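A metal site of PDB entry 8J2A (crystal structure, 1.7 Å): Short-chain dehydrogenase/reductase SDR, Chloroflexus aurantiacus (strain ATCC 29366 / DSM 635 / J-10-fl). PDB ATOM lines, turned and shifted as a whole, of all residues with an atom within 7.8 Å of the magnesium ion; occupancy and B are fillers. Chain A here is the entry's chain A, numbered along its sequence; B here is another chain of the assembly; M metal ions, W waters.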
ATOM      1  N   HIS A 445      20.767  -1.974 -15.639  1.00  0.00           N
ATOM      2  CA  HIS A 445      21.202  -0.892 -14.765  1.00  0.00           C
ATOM      3  C   HIS A 445      22.612  -1.152 -14.262  1.00  0.00           C
ATOM      4  O   HIS A 445      23.449  -0.251 -14.307  1.00  0.00           O
ATOM      5  CB  HIS A 445      20.221  -0.744 -13.584  1.00  0.00           C
ATOM      6  CG  HIS A 445      18.847  -0.338 -14.005  1.00  0.00           C
ATOM      7  ND1 HIS A 445      18.012  -1.201 -14.660  1.00  0.00           N
ATOM      8  CD2 HIS A 445      18.206   0.835 -13.798  1.00  0.00           C
ATOM      9  CE1 HIS A 445      16.871  -0.538 -14.831  1.00  0.00           C
ATOM     10  NE2 HIS A 445      16.952   0.695 -14.348  1.00  0.00           N
ATOM     11  N   PRO A 575      12.834  -0.862  -6.219  1.00  0.00           N
ATOM     12  CA  PRO A 575      12.459  -1.637  -7.417  1.00  0.00           C
ATOM     13  C   PRO A 575      12.079  -0.784  -8.618  1.00  0.00           C
ATOM     14  O   PRO A 575      11.601   0.344  -8.488  1.00  0.00           O
ATOM     15  CB  PRO A 575      11.230  -2.442  -6.948  1.00  0.00           C
ATOM     16  CG  PRO A 575      11.298  -2.466  -5.494  1.00  0.00           C
ATOM     17  CD  PRO A 575      12.000  -1.227  -5.054  1.00  0.00           C
ATOM     18  N   GLU A 576      12.200  -1.361  -9.800  1.00  0.00           N
ATOM     19  CA  GLU A 576      11.820  -0.680 -11.022  1.00  0.00           C
ATOM     20  C   GLU A 576      10.357  -0.966 -11.380  1.00  0.00           C
ATOM     21  O   GLU A 576       9.911  -2.120 -11.321  1.00  0.00           O
ATOM     22  CB  GLU A 576      12.776  -1.136 -12.153  1.00  0.00           C
ATOM     23  CG  GLU A 576      12.308  -0.821 -13.557  1.00  0.00           C
ATOM     24  CD  GLU A 576      13.138  -1.480 -14.650  1.00  0.00           C
ATOM     25  OE1 GLU A 576      13.174  -2.729 -14.707  1.00  0.00           O
ATOM     26  OE2 GLU A 576      13.709  -0.744 -15.477  1.00  0.00           O
ATOM     27  N   THR A 577       9.615   0.095 -11.720  1.00  0.00           N
ATOM     28  CA  THR A 577       8.277   0.033 -12.317  1.00  0.00           C
ATOM     29  C   THR A 577       8.455   0.540 -13.739  1.00  0.00           C
ATOM     30  O   THR A 577       9.344   1.371 -14.000  1.00  0.00           O
ATOM     31  CB  THR A 577       7.221   0.882 -11.588  1.00  0.00           C
ATOM     32  OG1 THR A 577       7.662   2.246 -11.455  1.00  0.00           O
ATOM     33  CG2 THR A 577       6.803   0.297 -10.268  1.00  0.00           C
ATOM     34  N   THR A 578       7.650   0.028 -14.664  1.00  0.00           N
ATOM     35  CA  THR A 578       7.660   0.428 -16.066  1.00  0.00           C
ATOM     36  C   THR A 578       6.210   0.671 -16.476  1.00  0.00           C
ATOM     37  O   THR A 578       5.297   0.398 -15.685  1.00  0.00           O
ATOM     38  CB  THR A 578       8.283  -0.680 -16.961  1.00  0.00           C
ATOM     39  OG1 THR A 578       7.424  -1.817 -16.963  1.00  0.00           O
ATOM     40  CG2 THR A 578       9.699  -1.089 -16.533  1.00  0.00           C
ATOM     41  N   ALA A 579       5.995   1.115 -17.731  1.00  0.00           N
ATOM     42  CA  ALA A 579       4.672   1.318 -18.316  1.00  0.00           C
ATOM     43  C   ALA A 579       3.871  -0.001 -18.366  1.00  0.00           C
ATOM     44  O   ALA A 579       2.644   0.049 -18.398  1.00  0.00           O
ATOM     45  CB  ALA A 579       4.820   1.872 -19.735  1.00  0.00           C
ATOM     46  N   SER A 581       4.376  -2.700 -15.933  1.00  0.00           N
ATOM     47  CA  SER A 581       4.380  -3.380 -14.625  1.00  0.00           C
ATOM     48  C   SER A 581       2.915  -3.634 -14.266  1.00  0.00           C
ATOM     49  O   SER A 581       2.057  -2.833 -14.669  1.00  0.00           O
ATOM     50  CB  SER A 581       5.009  -2.482 -13.563  1.00  0.00           C
ATOM     51  OG  SER A 581       6.410  -2.443 -13.717  1.00  0.00           O
ATOM     52  N   PHE A 586       2.959  -1.957  -9.089  1.00  0.00           N
ATOM     53  CA  PHE A 586       2.999  -0.527  -8.770  1.00  0.00           C
ATOM     54  C   PHE A 586       2.695  -0.275  -7.298  1.00  0.00           C
ATOM     55  O   PHE A 586       3.376   0.544  -6.675  1.00  0.00           O
ATOM     56  CB  PHE A 586       1.993   0.265  -9.610  1.00  0.00           C
ATOM     57  CG  PHE A 586       2.641   0.825 -10.846  1.00  0.00           C
ATOM     58  CD1 PHE A 586       3.404   1.996 -10.778  1.00  0.00           C
ATOM     59  CD2 PHE A 586       2.493   0.206 -12.077  1.00  0.00           C
ATOM     60  CE1 PHE A 586       4.016   2.509 -11.922  1.00  0.00           C
ATOM     61  CE2 PHE A 586       3.119   0.721 -13.218  1.00  0.00           C
ATOM     62  CZ  PHE A 586       3.861   1.869 -13.132  1.00  0.00           C
ATOM     63  N   ASP A 620      15.105   6.340  -6.510  1.00  0.00           N
ATOM     64  CA  ASP A 620      13.907   5.568  -6.787  1.00  0.00           C
ATOM     65  C   ASP A 620      13.680   5.304  -8.282  1.00  0.00           C
ATOM     66  O   ASP A 620      13.673   6.242  -9.082  1.00  0.00           O
ATOM     67  CB  ASP A 620      12.699   6.283  -6.157  1.00  0.00           C
ATOM     68  CG  ASP A 620      12.739   6.315  -4.627  1.00  0.00           C
ATOM     69  OD1 ASP A 620      13.022   5.280  -4.018  1.00  0.00           O
ATOM     70  OD2 ASP A 620      12.532   7.401  -4.056  1.00  0.00           O
ATOM     71  N   LEU A 621      13.463   4.029  -8.636  1.00  0.00           N
ATOM     72  CA  LEU A 621      13.146   3.608 -10.000  1.00  0.00           C
ATOM     73  C   LEU A 621      11.621   3.318 -10.052  1.00  0.00           C
ATOM     74  O   LEU A 621      11.125   2.724 -11.020  1.00  0.00           O
ATOM     75  CB  LEU A 621      13.918   2.305 -10.314  1.00  0.00           C
ATOM     76  CG  LEU A 621      15.433   2.402 -10.470  1.00  0.00           C
ATOM     77  CD1 LEU A 621      16.026   1.020 -10.756  1.00  0.00           C
ATOM     78  CD2 LEU A 621      15.805   3.352 -11.620  1.00  0.00           C
ATOM     79  N   THR A 622      10.916   3.653  -8.967  1.00  0.00           N
ATOM     80  CA  THR A 622       9.467   3.454  -8.761  1.00  0.00           C
ATOM     81  C   THR A 622       8.789   4.827  -8.896  1.00  0.00           C
ATOM     82  O   THR A 622       9.300   5.833  -8.392  1.00  0.00           O
ATOM     83  CB  THR A 622       9.221   2.895  -7.322  1.00  0.00           C
ATOM     84  OG1 THR A 622       9.590   1.504  -7.234  1.00  0.00           O
ATOM     85  CG2 THR A 622       7.758   3.045  -6.857  1.00  0.00           C
ATOM     86  N   ARG A 623       7.646   4.857  -9.582  1.00  0.00           N
ATOM     87  CA  ARG A 623       6.834   6.067  -9.713  1.00  0.00           C
ATOM     88  C   ARG A 623       5.446   5.733  -9.203  1.00  0.00           C
ATOM     89  O   ARG A 623       5.070   4.549  -9.141  1.00  0.00           O
ATOM     90  CB  ARG A 623       6.807   6.603 -11.151  1.00  0.00           C
ATOM     91  CG  ARG A 623       8.149   7.203 -11.581  1.00  0.00           C
ATOM     92  CD  ARG A 623       8.083   7.773 -12.981  1.00  0.00           C
ATOM     93  NE  ARG A 623       9.198   8.679 -13.242  1.00  0.00           N
ATOM     94  CZ  ARG A 623       9.158   9.997 -13.039  1.00  0.00           C
ATOM     95  NH1 ARG A 623       8.055  10.568 -12.570  1.00  0.00           N
ATOM     96  NH2 ARG A 623      10.220  10.743 -13.305  1.00  0.00           N
ATOM     97  N   GLU A 628       3.267   8.281 -15.862  1.00  0.00           N
ATOM     98  CA  GLU A 628       4.536   9.036 -15.746  1.00  0.00           C
ATOM     99  C   GLU A 628       5.712   8.305 -16.388  1.00  0.00           C
ATOM    100  O   GLU A 628       6.781   8.890 -16.580  1.00  0.00           O
ATOM    101  CB  GLU A 628       4.879   9.288 -14.284  1.00  0.00           C
ATOM    102  CG  GLU A 628       3.850  10.100 -13.510  1.00  0.00           C
ATOM    103  CD  GLU A 628       4.029  10.063 -12.011  1.00  0.00           C
ATOM    104  OE1 GLU A 628       5.164   9.791 -11.542  1.00  0.00           O
ATOM    105  OE2 GLU A 628       3.035  10.325 -11.278  1.00  0.00           O
ATOM    106  N   GLU A 629       5.537   7.015 -16.672  1.00  0.00           N
ATOM    107  CA  GLU A 629       6.577   6.151 -17.189  1.00  0.00           C
ATOM    108  C   GLU A 629       6.937   6.394 -18.679  1.00  0.00           C
ATOM    109  O   GLU A 629       6.042   6.768 -19.445  1.00  0.00           O
ATOM    110  CB  GLU A 629       6.144   4.675 -17.031  1.00  0.00           C
ATOM    111  CG  GLU A 629       5.984   4.220 -15.590  1.00  0.00           C
ATOM    112  CD  GLU A 629       7.265   4.069 -14.780  1.00  0.00           C
ATOM    113  OE1 GLU A 629       8.363   4.075 -15.381  1.00  0.00           O
ATOM    114  OE2 GLU A 629       7.156   3.908 -13.543  1.00  0.00           O
ATOM    115  N   PRO A 630       8.189   6.068 -19.096  1.00  0.00           N
ATOM    116  CA  PRO A 630       8.534   6.167 -20.536  1.00  0.00           C
ATOM    117  C   PRO A 630       7.669   5.220 -21.384  1.00  0.00           C
ATOM    118  O   PRO A 630       7.327   4.119 -20.922  1.00  0.00           O
ATOM    119  CB  PRO A 630       9.998   5.729 -20.574  1.00  0.00           C
ATOM    120  CG  PRO A 630      10.507   5.897 -19.212  1.00  0.00           C
ATOM    121  CD  PRO A 630       9.342   5.594 -18.309  1.00  0.00           C
ATOM    122  N   ARG A 636      12.837   5.822 -22.821  1.00  0.00           N
ATOM    123  CA  ARG A 636      13.522   4.788 -22.045  1.00  0.00           C
ATOM    124  C   ARG A 636      15.015   5.112 -21.960  1.00  0.00           C
ATOM    125  O   ARG A 636      15.607   4.942 -20.897  1.00  0.00           O
ATOM    126  CB  ARG A 636      13.253   3.375 -22.633  1.00  0.00           C
ATOM    127  CG  ARG A 636      14.103   2.217 -22.051  1.00  0.00           C
ATOM    128  CD  ARG A 636      13.876   1.954 -20.555  1.00  0.00           C
ATOM    129  NE  ARG A 636      14.583   0.754 -20.089  1.00  0.00           N
ATOM    130  CZ  ARG A 636      14.527   0.258 -18.855  1.00  0.00           C
ATOM    131  NH1 ARG A 636      13.813   0.885 -17.918  1.00  0.00           N
ATOM    132  NH2 ARG A 636      15.179  -0.848 -18.543  1.00  0.00           N
ATOM    133  N   GLU A 639      15.371   7.826 -19.462  1.00  0.00           N
ATOM    134  CA  GLU A 639      15.191   7.309 -18.112  1.00  0.00           C
ATOM    135  C   GLU A 639      16.480   6.645 -17.590  1.00  0.00           C
ATOM    136  O   GLU A 639      16.885   6.920 -16.461  1.00  0.00           O
ATOM    137  CB  GLU A 639      14.040   6.298 -18.075  1.00  0.00           C
ATOM    138  CG  GLU A 639      13.726   5.800 -16.679  1.00  0.00           C
ATOM    139  CD  GLU A 639      12.655   4.740 -16.646  1.00  0.00           C
ATOM    140  OE1 GLU A 639      12.796   3.737 -17.388  1.00  0.00           O
ATOM    141  OE2 GLU A 639      11.665   4.912 -15.895  1.00  0.00           O
ATOM    142  N   VAL A 674      13.775   8.852 -10.346  1.00  0.00           N
ATOM    143  CA  VAL A 674      14.223   8.815 -11.746  1.00  0.00           C
ATOM    144  C   VAL A 674      12.966   8.900 -12.640  1.00  0.00           C
ATOM    145  O   VAL A 674      12.931   9.774 -13.525  1.00  0.00           O
ATOM    146  CB  VAL A 674      15.049   7.540 -12.016  1.00  0.00           C
ATOM    147  CG1 VAL A 674      15.420   7.431 -13.502  1.00  0.00           C
ATOM    148  CG2 VAL A 674      16.298   7.495 -11.157  1.00  0.00           C
ATOM    149  OXT VAL A 674      12.046   8.065 -12.456  1.00  0.00           O
ATOM    150  N   TYR B 662       7.758  12.496 -21.772  1.00  0.00           N
ATOM    151  CA  TYR B 662       8.373  12.063 -20.499  1.00  0.00           C
ATOM    152  C   TYR B 662       9.210  13.191 -19.885  1.00  0.00           C
ATOM    153  O   TYR B 662       8.979  13.568 -18.727  1.00  0.00           O
ATOM    154  CB  TYR B 662       9.218  10.781 -20.744  1.00  0.00           C
ATOM    155  CG  TYR B 662      10.126  10.365 -19.599  1.00  0.00           C
ATOM    156  CD1 TYR B 662       9.605   9.776 -18.452  1.00  0.00           C
ATOM    157  CD2 TYR B 662      11.512  10.493 -19.702  1.00  0.00           C
ATOM    158  CE1 TYR B 662      10.435   9.360 -17.412  1.00  0.00           C
ATOM    159  CE2 TYR B 662      12.348  10.087 -18.667  1.00  0.00           C
ATOM    160  CZ  TYR B 662      11.806   9.505 -17.530  1.00  0.00           C
ATOM    161  OH  TYR B 662      12.639   9.120 -16.495  1.00  0.00           O
HETATM  162 MG    MG M   1      10.319   3.274 -14.957  1.00  0.00          MG
HETATM  163  O   HOH W   1      10.812   2.073 -16.704  1.00  0.00           O
HETATM  164  O   HOH W   2       9.722   4.395 -12.891  1.00  0.00           O
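Water W1 bridges OE1 of Glu 639 (2.7 Å) and NH1 of Arg 636 (3.4 Å). Water W2 lies within hydrogen-bond range of the side-chain carboxylate (OE2) of Glu 629, the backbone carbonyl oxygen (O) of Leu 621 and the side-chain hydroxyl (OG1) of Thr 577.
The side-chain hydroxyl of Thr 577 lies within hydrogen-bond range of the backbone NH of Arg 623 (3.2 Å). NH1 of Arg 636 is in salt-bridge range of OE1 of Glu 639, 3.1 Å away. The backbone NH (N) of Thr 577 is in hydrogen-bond range of the backbone carbonyl oxygen (O) of Leu 621 (3.1 Å).
Of the 19 residues printed, 3 come within 4 Å of the magnesium ion. The nearest printed residue that does not touch the magnesium ion is Thr 578 (4.05 Å).
The side-chain carboxylate (OE1) of Glu 629 binds the magnesium ion, 2.2 Å away. Water W1 is bound to the magnesium ion (2.2 Å). OE2 of Glu 639 is bound to the magnesium ion, 2.3 Å away. O of Thr 577 is bound to the magnesium ion (2.3 Å). Water W2 binds the magnesium ion (2.4 Å). The magnesium ion has five donor atoms within binding distance.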
